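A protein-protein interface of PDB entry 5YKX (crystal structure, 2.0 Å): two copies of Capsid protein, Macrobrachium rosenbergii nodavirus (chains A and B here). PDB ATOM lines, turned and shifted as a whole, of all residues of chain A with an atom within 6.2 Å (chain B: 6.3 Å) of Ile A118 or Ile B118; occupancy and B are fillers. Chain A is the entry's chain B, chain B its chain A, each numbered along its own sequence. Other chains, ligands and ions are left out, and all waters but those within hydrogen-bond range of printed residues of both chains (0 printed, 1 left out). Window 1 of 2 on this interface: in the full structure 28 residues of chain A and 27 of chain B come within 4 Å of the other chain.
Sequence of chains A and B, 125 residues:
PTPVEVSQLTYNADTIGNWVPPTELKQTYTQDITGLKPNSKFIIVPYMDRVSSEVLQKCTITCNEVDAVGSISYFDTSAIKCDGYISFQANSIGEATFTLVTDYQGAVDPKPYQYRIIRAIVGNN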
ATOM      1  N   TYR A  11     -19.006  14.808 -35.049  1.00  0.00           N
ATOM      2  CA  TYR A  11     -19.402  14.775 -33.650  1.00  0.00           C
ATOM      3  C   TYR A  11     -18.884  13.446 -33.105  1.00  0.00           C
ATOM      4  O   TYR A  11     -19.038  12.389 -33.740  1.00  0.00           O
ATOM      5  CB  TYR A  11     -20.917  14.869 -33.495  1.00  0.00           C
ATOM      6  CG  TYR A  11     -21.527  16.151 -33.978  1.00  0.00           C
ATOM      7  CD1 TYR A  11     -21.676  17.247 -33.120  1.00  0.00           C
ATOM      8  CD2 TYR A  11     -21.984  16.274 -35.288  1.00  0.00           C
ATOM      9  CE1 TYR A  11     -22.252  18.417 -33.543  1.00  0.00           C
ATOM     10  CE2 TYR A  11     -22.554  17.466 -35.719  1.00  0.00           C
ATOM     11  CZ  TYR A  11     -22.666  18.519 -34.875  1.00  0.00           C
ATOM     12  OH  TYR A  11     -23.292  19.665 -35.263  1.00  0.00           O
ATOM     13  N   ASN A  12     -18.216  13.495 -31.978  1.00  0.00           N
ATOM     14  CA  ASN A  12     -17.897  12.271 -31.286  1.00  0.00           C
ATOM     15  C   ASN A  12     -18.939  12.110 -30.202  1.00  0.00           C
ATOM     16  O   ASN A  12     -19.104  13.004 -29.363  1.00  0.00           O
ATOM     17  CB  ASN A  12     -16.515  12.295 -30.620  1.00  0.00           C
ATOM     18  CG  ASN A  12     -16.152  10.925 -29.972  1.00  0.00           C
ATOM     19  OD1 ASN A  12     -16.819   9.895 -30.133  1.00  0.00           O
ATOM     20  ND2 ASN A  12     -15.055  10.919 -29.262  1.00  0.00           N
ATOM     21  N   ALA A  13     -19.579  10.963 -30.181  1.00  0.00           N
ATOM     22  CA  ALA A  13     -20.703  10.712 -29.246  1.00  0.00           C
ATOM     23  C   ALA A  13     -20.576   9.332 -28.597  1.00  0.00           C
ATOM     24  O   ALA A  13     -21.525   8.829 -28.016  1.00  0.00           O
ATOM     25  CB  ALA A  13     -22.023  10.825 -30.002  1.00  0.00           C
ATOM     26  N   THR A  15     -18.475   8.472 -26.030  1.00  0.00           N
ATOM     27  CA  THR A  15     -18.196   8.450 -24.566  1.00  0.00           C
ATOM     28  C   THR A  15     -19.478   8.337 -23.774  1.00  0.00           C
ATOM     29  O   THR A  15     -20.353   9.206 -23.833  1.00  0.00           O
ATOM     30  CB  THR A  15     -17.531   9.751 -24.136  1.00  0.00           C
ATOM     31  OG1 THR A  15     -16.380   9.862 -24.929  1.00  0.00           O
ATOM     32  CG2 THR A  15     -17.126   9.776 -22.676  1.00  0.00           C
ATOM     33  N   LYS A  41     -15.662  22.395 -25.343  1.00  0.00           N
ATOM     34  CA  LYS A  41     -17.083  22.568 -25.135  1.00  0.00           C
ATOM     35  C   LYS A  41     -17.756  21.238 -25.520  1.00  0.00           C
ATOM     36  O   LYS A  41     -17.451  20.611 -26.584  1.00  0.00           O
ATOM     37  CB  LYS A  41     -17.671  23.659 -26.000  1.00  0.00           C
ATOM     38  CG  LYS A  41     -16.959  25.011 -25.973  1.00  0.00           C
ATOM     39  CD  LYS A  41     -17.207  25.690 -24.695  1.00  0.00           C
ATOM     40  CE  LYS A  41     -16.815  27.156 -24.824  1.00  0.00           C
ATOM     41  NZ  LYS A  41     -17.689  27.879 -25.795  1.00  0.00           N
ATOM     42  N   PHE A  42     -18.620  20.801 -24.620  1.00  0.00           N
ATOM     43  CA  PHE A  42     -19.313  19.536 -24.746  1.00  0.00           C
ATOM     44  C   PHE A  42     -20.811  19.742 -24.465  1.00  0.00           C
ATOM     45  O   PHE A  42     -21.246  20.725 -23.888  1.00  0.00           O
ATOM     46  CB  PHE A  42     -18.843  18.562 -23.699  1.00  0.00           C
ATOM     47  CG  PHE A  42     -17.419  18.244 -23.756  1.00  0.00           C
ATOM     48  CD1 PHE A  42     -16.965  17.201 -24.485  1.00  0.00           C
ATOM     49  CD2 PHE A  42     -16.509  19.064 -23.076  1.00  0.00           C
ATOM     50  CE1 PHE A  42     -15.627  16.924 -24.575  1.00  0.00           C
ATOM     51  CE2 PHE A  42     -15.181  18.755 -23.150  1.00  0.00           C
ATOM     52  CZ  PHE A  42     -14.746  17.708 -23.877  1.00  0.00           C
ATOM     53  N   ILE A  43     -21.576  18.728 -24.808  1.00  0.00           N
ATOM     54  CA  ILE A  43     -22.946  18.619 -24.304  1.00  0.00           C
ATOM     55  C   ILE A  43     -23.152  17.230 -23.816  1.00  0.00           C
ATOM     56  O   ILE A  43     -22.791  16.271 -24.528  1.00  0.00           O
ATOM     57  CB  ILE A  43     -23.936  19.046 -25.356  1.00  0.00           C
ATOM     58  CG1 ILE A  43     -25.375  18.995 -24.820  1.00  0.00           C
ATOM     59  CG2 ILE A  43     -23.776  18.303 -26.653  1.00  0.00           C
ATOM     60  CD1 ILE A  43     -26.277  19.756 -25.765  1.00  0.00           C
ATOM     61  N   ILE A  44     -23.713  17.121 -22.617  1.00  0.00           N
ATOM     62  CA  ILE A  44     -24.026  15.784 -22.030  1.00  0.00           C
ATOM     63  C   ILE A  44     -25.515  15.574 -22.118  1.00  0.00           C
ATOM     64  O   ILE A  44     -26.270  16.498 -21.864  1.00  0.00           O
ATOM     65  CB  ILE A  44     -23.456  15.614 -20.611  1.00  0.00           C
ATOM     66  CG1 ILE A  44     -23.789  14.305 -19.975  1.00  0.00           C
ATOM     67  CG2 ILE A  44     -23.908  16.677 -19.686  1.00  0.00           C
ATOM     68  CD1 ILE A  44     -22.858  14.067 -18.746  1.00  0.00           C
ATOM     69  N   VAL A  45     -25.904  14.400 -22.627  1.00  0.00           N
ATOM     70  CA  VAL A  45     -27.289  14.042 -22.764  1.00  0.00           C
ATOM     71  C   VAL A  45     -27.532  12.700 -22.064  1.00  0.00           C
ATOM     72  O   VAL A  45     -26.623  11.863 -21.956  1.00  0.00           O
ATOM     73  CB  VAL A  45     -27.752  13.973 -24.239  1.00  0.00           C
ATOM     74  CG1 VAL A  45     -27.592  15.299 -24.964  1.00  0.00           C
ATOM     75  CG2 VAL A  45     -27.010  12.877 -24.984  1.00  0.00           C
ATOM     76  N   ARG A 116     -24.247  10.177 -22.014  1.00  0.00           N
ATOM     77  CA  ARG A 116     -23.525  10.163 -23.226  1.00  0.00           C
ATOM     78  C   ARG A 116     -22.937  11.584 -23.384  1.00  0.00           C
ATOM     79  O   ARG A 116     -23.662  12.541 -23.299  1.00  0.00           O
ATOM     80  CB  ARG A 116     -24.410   9.820 -24.434  1.00  0.00           C
ATOM     81  CG  ARG A 116     -23.691   9.885 -25.778  1.00  0.00           C
ATOM     82  CD  ARG A 116     -24.580   9.517 -26.964  1.00  0.00           C
ATOM     83  NE  ARG A 116     -25.274   8.276 -26.771  1.00  0.00           N
ATOM     84  CZ  ARG A 116     -24.793   7.062 -26.928  1.00  0.00           C
ATOM     85  NH1 ARG A 116     -23.572   6.871 -27.320  1.00  0.00           N
ATOM     86  NH2 ARG A 116     -25.567   6.032 -26.623  1.00  0.00           N
ATOM     87  N   ILE A 117     -21.651  11.683 -23.687  1.00  0.00           N
ATOM     88  CA  ILE A 117     -21.003  13.005 -23.867  1.00  0.00           C
ATOM     89  C   ILE A 117     -20.723  13.224 -25.337  1.00  0.00           C
ATOM     90  O   ILE A 117     -20.120  12.393 -25.990  1.00  0.00           O
ATOM     91  CB  ILE A 117     -19.679  13.120 -23.099  1.00  0.00           C
ATOM     92  CG1 ILE A 117     -19.913  12.801 -21.607  1.00  0.00           C
ATOM     93  CG2 ILE A 117     -18.985  14.463 -23.280  1.00  0.00           C
ATOM     94  CD1 ILE A 117     -18.654  12.902 -20.767  1.00  0.00           C
ATOM     95  N   ILE A 118     -21.159  14.364 -25.847  1.00  0.00           N
ATOM     96  CA  ILE A 118     -20.982  14.641 -27.251  1.00  0.00           C
ATOM     97  C   ILE A 118     -19.995  15.824 -27.387  1.00  0.00           C
ATOM     98  O   ILE A 118     -20.113  16.810 -26.677  1.00  0.00           O
ATOM     99  CB  ILE A 118     -22.285  15.061 -27.846  1.00  0.00           C
ATOM    100  CG1 ILE A 118     -23.237  13.859 -27.812  1.00  0.00           C
ATOM    101  CG2 ILE A 118     -22.115  15.642 -29.266  1.00  0.00           C
ATOM    102  CD1 ILE A 118     -24.645  14.259 -28.055  1.00  0.00           C
ATOM    103  N   ARG A 119     -19.068  15.657 -28.301  1.00  0.00           N
ATOM    104  CA  ARG A 119     -18.068  16.683 -28.622  1.00  0.00           C
ATOM    105  C   ARG A 119     -18.010  16.912 -30.119  1.00  0.00           C
ATOM    106  O   ARG A 119     -17.807  15.999 -30.889  1.00  0.00           O
ATOM    107  CB  ARG A 119     -16.710  16.264 -28.074  1.00  0.00           C
ATOM    108  CG  ARG A 119     -15.523  17.179 -28.354  1.00  0.00           C
ATOM    109  CD  ARG A 119     -14.214  16.362 -28.179  1.00  0.00           C
ATOM    110  NE  ARG A 119     -13.096  17.019 -28.838  1.00  0.00           N
ATOM    111  CZ  ARG A 119     -12.018  16.409 -29.284  1.00  0.00           C
ATOM    112  NH1 ARG A 119     -11.105  17.098 -29.947  1.00  0.00           N
ATOM    113  NH2 ARG A 119     -11.841  15.115 -29.077  1.00  0.00           N
ATOM    114  N   ALA A 120     -18.238  18.159 -30.493  1.00  0.00           N
ATOM    115  CA  ALA A 120     -17.993  18.596 -31.907  1.00  0.00           C
ATOM    116  C   ALA A 120     -16.453  18.712 -32.108  1.00  0.00           C
ATOM    117  O   ALA A 120     -15.754  19.481 -31.375  1.00  0.00           O
ATOM    118  CB  ALA A 120     -18.624  19.911 -32.159  1.00  0.00           C
ATOM    119  N   TYR B  11     -23.468  25.018 -28.546  1.00  0.00           N
ATOM    120  CA  TYR B  11     -24.351  24.005 -29.094  1.00  0.00           C
ATOM    121  C   TYR B  11     -25.748  24.567 -29.050  1.00  0.00           C
ATOM    122  O   TYR B  11     -26.118  25.178 -28.081  1.00  0.00           O
ATOM    123  CB  TYR B  11     -24.240  22.744 -28.277  1.00  0.00           C
ATOM    124  CG  TYR B  11     -22.910  22.076 -28.381  1.00  0.00           C
ATOM    125  CD1 TYR B  11     -22.593  21.229 -29.430  1.00  0.00           C
ATOM    126  CD2 TYR B  11     -21.977  22.237 -27.367  1.00  0.00           C
ATOM    127  CE1 TYR B  11     -21.363  20.602 -29.481  1.00  0.00           C
ATOM    128  CE2 TYR B  11     -20.731  21.631 -27.425  1.00  0.00           C
ATOM    129  CZ  TYR B  11     -20.418  20.829 -28.464  1.00  0.00           C
ATOM    130  OH  TYR B  11     -19.220  20.160 -28.462  1.00  0.00           O
ATOM    131  N   ASN B  12     -26.539  24.355 -30.056  1.00  0.00           N
ATOM    132  CA  ASN B  12     -28.004  24.457 -29.836  1.00  0.00           C
ATOM    133  C   ASN B  12     -28.570  23.011 -29.747  1.00  0.00           C
ATOM    134  O   ASN B  12     -28.313  22.195 -30.647  1.00  0.00           O
ATOM    135  CB  ASN B  12     -28.666  25.169 -30.980  1.00  0.00           C
ATOM    136  CG  ASN B  12     -30.180  25.296 -30.806  1.00  0.00           C
ATOM    137  OD1 ASN B  12     -30.781  25.388 -29.685  1.00  0.00           O
ATOM    138  ND2 ASN B  12     -30.819  25.341 -31.923  1.00  0.00           N
ATOM    139  N   ALA B  13     -29.319  22.751 -28.700  1.00  0.00           N
ATOM    140  CA  ALA B  13     -29.955  21.440 -28.434  1.00  0.00           C
ATOM    141  C   ALA B  13     -31.425  21.575 -28.104  1.00  0.00           C
ATOM    142  O   ALA B  13     -32.043  20.653 -27.566  1.00  0.00           O
ATOM    143  CB  ALA B  13     -29.177  20.751 -27.309  1.00  0.00           C
ATOM    144  N   THR B  15     -33.989  22.040 -30.410  1.00  0.00           N
ATOM    145  CA  THR B  15     -34.846  21.556 -31.448  1.00  0.00           C
ATOM    146  C   THR B  15     -35.284  20.121 -31.080  1.00  0.00           C
ATOM    147  O   THR B  15     -34.444  19.219 -31.012  1.00  0.00           O
ATOM    148  CB  THR B  15     -34.172  21.538 -32.813  1.00  0.00           C
ATOM    149  OG1 THR B  15     -33.757  22.894 -33.118  1.00  0.00           O
ATOM    150  CG2 THR B  15     -35.123  21.008 -33.916  1.00  0.00           C
ATOM    151  N   LYS B  41     -24.124  20.200 -40.424  1.00  0.00           N
ATOM    152  CA  LYS B  41     -23.885  18.891 -39.776  1.00  0.00           C
ATOM    153  C   LYS B  41     -24.479  18.881 -38.417  1.00  0.00           C
ATOM    154  O   LYS B  41     -24.282  19.814 -37.602  1.00  0.00           O
ATOM    155  CB  LYS B  41     -22.396  18.602 -39.685  1.00  0.00           C
ATOM    156  CG  LYS B  41     -21.902  18.323 -41.098  1.00  0.00           C
ATOM    157  CD  LYS B  41     -20.413  18.280 -41.256  1.00  0.00           C
ATOM    158  CE  LYS B  41     -20.076  17.456 -42.495  1.00  0.00           C
ATOM    159  NZ  LYS B  41     -18.711  17.807 -42.917  1.00  0.00           N
ATOM    160  N   PHE B  42     -25.179  17.795 -38.142  1.00  0.00           N
ATOM    161  CA  PHE B  42     -25.969  17.657 -36.918  1.00  0.00           C
ATOM    162  C   PHE B  42     -25.758  16.284 -36.305  1.00  0.00           C
ATOM    163  O   PHE B  42     -25.304  15.372 -36.981  1.00  0.00           O
ATOM    164  CB  PHE B  42     -27.497  17.664 -37.278  1.00  0.00           C
ATOM    165  CG  PHE B  42     -27.961  18.955 -37.898  1.00  0.00           C
ATOM    166  CD1 PHE B  42     -28.398  20.007 -37.089  1.00  0.00           C
ATOM    167  CD2 PHE B  42     -27.882  19.143 -39.289  1.00  0.00           C
ATOM    168  CE1 PHE B  42     -28.732  21.223 -37.632  1.00  0.00           C
ATOM    169  CE2 PHE B  42     -28.273  20.366 -39.840  1.00  0.00           C
ATOM    170  CZ  PHE B  42     -28.725  21.375 -39.035  1.00  0.00           C
ATOM    171  N   ILE B  43     -26.193  16.131 -35.057  1.00  0.00           N
ATOM    172  CA  ILE B  43     -26.324  14.827 -34.443  1.00  0.00           C
ATOM    173  C   ILE B  43     -27.697  14.810 -33.800  1.00  0.00           C
ATOM    174  O   ILE B  43     -28.087  15.771 -33.063  1.00  0.00           O
ATOM    175  CB  ILE B  43     -25.150  14.500 -33.471  1.00  0.00           C
ATOM    176  CG1 ILE B  43     -25.325  13.083 -32.863  1.00  0.00           C
ATOM    177  CG2 ILE B  43     -25.025  15.553 -32.395  1.00  0.00           C
ATOM    178  CD1 ILE B  43     -24.093  12.621 -32.105  1.00  0.00           C
ATOM    179  N   ILE B  44     -28.460  13.765 -34.114  1.00  0.00           N
ATOM    180  CA  ILE B  44     -29.770  13.610 -33.558  1.00  0.00           C
ATOM    181  C   ILE B  44     -29.675  12.511 -32.496  1.00  0.00           C
ATOM    182  O   ILE B  44     -29.071  11.433 -32.741  1.00  0.00           O
ATOM    183  CB  ILE B  44     -30.782  13.285 -34.667  1.00  0.00           C
ATOM    184  CG1 ILE B  44     -32.218  13.092 -34.156  1.00  0.00           C
ATOM    185  CG2 ILE B  44     -30.369  12.073 -35.527  1.00  0.00           C
ATOM    186  CD1 ILE B  44     -33.280  13.236 -35.270  1.00  0.00           C
ATOM    187  N   VAL B  45     -30.257  12.763 -31.328  1.00  0.00           N
ATOM    188  CA  VAL B  45     -30.297  11.776 -30.234  1.00  0.00           C
ATOM    189  C   VAL B  45     -31.740  11.526 -29.809  1.00  0.00           C
ATOM    190  O   VAL B  45     -32.588  12.418 -29.969  1.00  0.00           O
ATOM    191  CB  VAL B  45     -29.482  12.223 -29.037  1.00  0.00           C
ATOM    192  CG1 VAL B  45     -28.022  12.406 -29.481  1.00  0.00           C
ATOM    193  CG2 VAL B  45     -30.045  13.475 -28.399  1.00  0.00           C
ATOM    194  N   TYR B  85     -27.558   7.195 -31.633  1.00  0.00           N
ATOM    195  CA  TYR B  85     -27.448   8.519 -32.144  1.00  0.00           C
ATOM    196  C   TYR B  85     -27.266   8.397 -33.642  1.00  0.00           C
ATOM    197  O   TYR B  85     -26.857   7.332 -34.116  1.00  0.00           O
ATOM    198  CB  TYR B  85     -26.332   9.365 -31.485  1.00  0.00           C
ATOM    199  CG  TYR B  85     -24.966   8.757 -31.738  1.00  0.00           C
ATOM    200  CD1 TYR B  85     -24.380   7.890 -30.796  1.00  0.00           C
ATOM    201  CD2 TYR B  85     -24.305   8.975 -32.928  1.00  0.00           C
ATOM    202  CE1 TYR B  85     -23.127   7.313 -30.999  1.00  0.00           C
ATOM    203  CE2 TYR B  85     -23.085   8.366 -33.162  1.00  0.00           C
ATOM    204  CZ  TYR B  85     -22.519   7.537 -32.172  1.00  0.00           C
ATOM    205  OH  TYR B  85     -21.293   6.980 -32.392  1.00  0.00           O
ATOM    206  N   ARG B 116     -34.213  14.772 -30.305  1.00  0.00           N
ATOM    207  CA  ARG B 116     -33.601  16.038 -30.057  1.00  0.00           C
ATOM    208  C   ARG B 116     -32.446  16.199 -31.062  1.00  0.00           C
ATOM    209  O   ARG B 116     -31.587  15.326 -31.205  1.00  0.00           O
ATOM    210  CB  ARG B 116     -33.012  16.117 -28.687  1.00  0.00           C
ATOM    211  CG  ARG B 116     -32.375  17.439 -28.350  1.00  0.00           C
ATOM    212  CD  ARG B 116     -31.791  17.447 -26.918  1.00  0.00           C
ATOM    213  NE  ARG B 116     -32.734  17.076 -25.911  1.00  0.00           N
ATOM    214  CZ  ARG B 116     -33.631  17.861 -25.410  1.00  0.00           C
ATOM    215  NH1 ARG B 116     -33.705  19.146 -25.782  1.00  0.00           N
ATOM    216  NH2 ARG B 116     -34.497  17.345 -24.562  1.00  0.00           N
ATOM    217  N   ILE B 117     -32.415  17.329 -31.728  1.00  0.00           N
ATOM    218  CA  ILE B 117     -31.339  17.605 -32.728  1.00  0.00           C
ATOM    219  C   ILE B 117     -30.354  18.604 -32.142  1.00  0.00           C
ATOM    220  O   ILE B 117     -30.741  19.648 -31.615  1.00  0.00           O
ATOM    221  CB  ILE B 117     -31.923  18.206 -34.003  1.00  0.00           C
ATOM    222  CG1 ILE B 117     -32.894  17.186 -34.627  1.00  0.00           C
ATOM    223  CG2 ILE B 117     -30.799  18.455 -35.004  1.00  0.00           C
ATOM    224  CD1 ILE B 117     -33.552  17.597 -35.889  1.00  0.00           C
ATOM    225  N   ILE B 118     -29.094  18.247 -32.218  1.00  0.00           N
ATOM    226  CA  ILE B 118     -27.983  19.035 -31.714  1.00  0.00           C
ATOM    227  C   ILE B 118     -27.178  19.560 -32.869  1.00  0.00           C
ATOM    228  O   ILE B 118     -26.830  18.839 -33.777  1.00  0.00           O
ATOM    229  CB  ILE B 118     -27.098  18.176 -30.805  1.00  0.00           C
ATOM    230  CG1 ILE B 118     -27.962  17.765 -29.612  1.00  0.00           C
ATOM    231  CG2 ILE B 118     -25.924  18.958 -30.258  1.00  0.00           C
ATOM    232  CD1 ILE B 118     -27.344  16.754 -28.734  1.00  0.00           C
ATOM    233  N   ARG B 119     -26.930  20.846 -32.842  1.00  0.00           N
ATOM    234  CA  ARG B 119     -26.122  21.527 -33.873  1.00  0.00           C
ATOM    235  C   ARG B 119     -25.015  22.331 -33.175  1.00  0.00           C
ATOM    236  O   ARG B 119     -25.304  23.191 -32.301  1.00  0.00           O
ATOM    237  CB  ARG B 119     -27.021  22.507 -34.598  1.00  0.00           C
ATOM    238  CG  ARG B 119     -26.393  23.394 -35.667  1.00  0.00           C
ATOM    239  CD  ARG B 119     -27.438  24.392 -36.271  1.00  0.00           C
ATOM    240  NE  ARG B 119     -26.763  25.511 -36.955  1.00  0.00           N
ATOM    241  CZ  ARG B 119     -27.132  26.771 -36.887  1.00  0.00           C
ATOM    242  NH1 ARG B 119     -26.420  27.691 -37.500  1.00  0.00           N
ATOM    243  NH2 ARG B 119     -28.232  27.126 -36.257  1.00  0.00           N
ATOM    244  N   ALA B 120     -23.814  22.131 -33.652  1.00  0.00           N
ATOM    245  CA  ALA B 120     -22.657  22.941 -33.287  1.00  0.00           C
ATOM    246  C   ALA B 120     -22.718  24.246 -34.083  1.00  0.00           C
ATOM    247  O   ALA B 120     -22.700  24.218 -35.330  1.00  0.00           O
ATOM    248  CB  ALA B 120     -21.418  22.208 -33.624  1.00  0.00           C
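O of Lys A41 lies within hydrogen-bond range of OH of Tyr B11, at 2.6 Å.
O of Lys B41 sits at hydrogen-bond distance from OH of Tyr A11 (2.5 Å).
N of Ala A120 sits at hydrogen-bond distance from OH of Tyr B11, 3.0 Å away.
The side-chain hydroxyl of Tyr A11 sits at hydrogen-bond distance from the backbone NH of Ala B120 (3.0 Å).
The guanidinium group (NH1) of Arg B116 sits at hydrogen-bond distance from the backbone carbonyl oxygen (O) of Ala B13 (2.9 Å).
O of Val A45 is in hydrogen-bond range of N of Arg A116.
O of Arg B119 is in hydrogen-bond range of N of Asn B12, at 2.8 Å.
The backbone carbonyl oxygen (O) of Arg A119 is in hydrogen-bond range of the backbone NH (N) of Asn A12, 2.8 Å away.
O of Ile B43 sits at hydrogen-bond distance from N of Ile B118 (2.8 Å).
NH1 of Arg A116 sits at hydrogen-bond distance from O of Ala A13 (2.9 Å).
Tyr A11 touches Phe B42.
O of Ile B118 touches OH of Tyr A11, 3.9 Å away.
CA of Arg B119 touches OH of Tyr A11, 3.7 Å away.
Ile B43 touches Ala A13.
O of Ala A13 touches CE1 of Tyr B85 (3.7 Å).
C of Phe A42 touches CE2 of Tyr B11 (3.5 Å).
Ile A43 touches Ala B13 (CD1 to CB, 3.4 Å).
NH1 of Arg A116 touches CD1 of Tyr B85 (3.7 Å).
Ile A118 touches Ile B118 (CD1 to CD1, 3.7 Å).
Ala B120 touches Ala A120 (CB to CB, 3.9 Å).
Ile B118 touches just these residues of chain A: Tyr A11 (3.9 Å) and Ile A118 (3.7 Å).
Of the printed residues of chain A, Tyr B11 touches Lys A41, Phe A42, Ile A43, Ile A118, Arg A119 and Ala A120.
Of the printed residues of chain A, Tyr B85 touches Ala A13 (3.7 Å) and Arg A116 (3.7 Å).
The nearest residue of chain B that does not touch Ile A118 is Val B45 (4.1 Å).
The nearest residue of chain A that does not touch Ile B118 is Val A45 (4.05 Å).
Printed residues of chain A that touch a printed residue of chain B: Tyr A11, Ala A13, Lys A41, Phe A42, Ile A43, Arg A116, Ile A118, Arg A119 and Ala A120.
Hydrophobic or aromatic side chains of chain A that line the printed part of chain B: Tyr A11, Ala A13, Ile A43, Ile A118 and Ala A120.
Of the 15 printed residues of chain B, 9 touch a printed residue of chain A.
Printed residues of chain B that touch a printed residue of chain A: Tyr B11, Ala B13, Lys B41, Phe B42, Ile B43, Tyr B85, Ile B118, Arg B119 and Ala B120.
Hydrophobic or aromatic side chains of chain B that line the printed part of chain A: Tyr B11, Ala B13, Ile B43, Tyr B85, Ile B118 and Ala B120.
Among the printed residues, no Asp or Glu carboxylate lies within 4 Å of a Lys or Arg side-chain nitrogen of the other chain.
Tyr A11 touches Lys B41, and with the chains exchanged Lys A41 touches Tyr B11.
Tyr A11 touches Phe B42, and with the chains exchanged Phe A42 touches Tyr B11.
Tyr A11 touches Arg B119, and with the chains exchanged Arg A119 touches Tyr B11.
Tyr A11 touches Ala B120, and with the chains exchanged Ala A120 touches Tyr B11.
14 positions are printed for both chains.
Of the 18 pairs that touch across the chains among the printed residues, 16 have their exchanged pair printed and touching as well.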
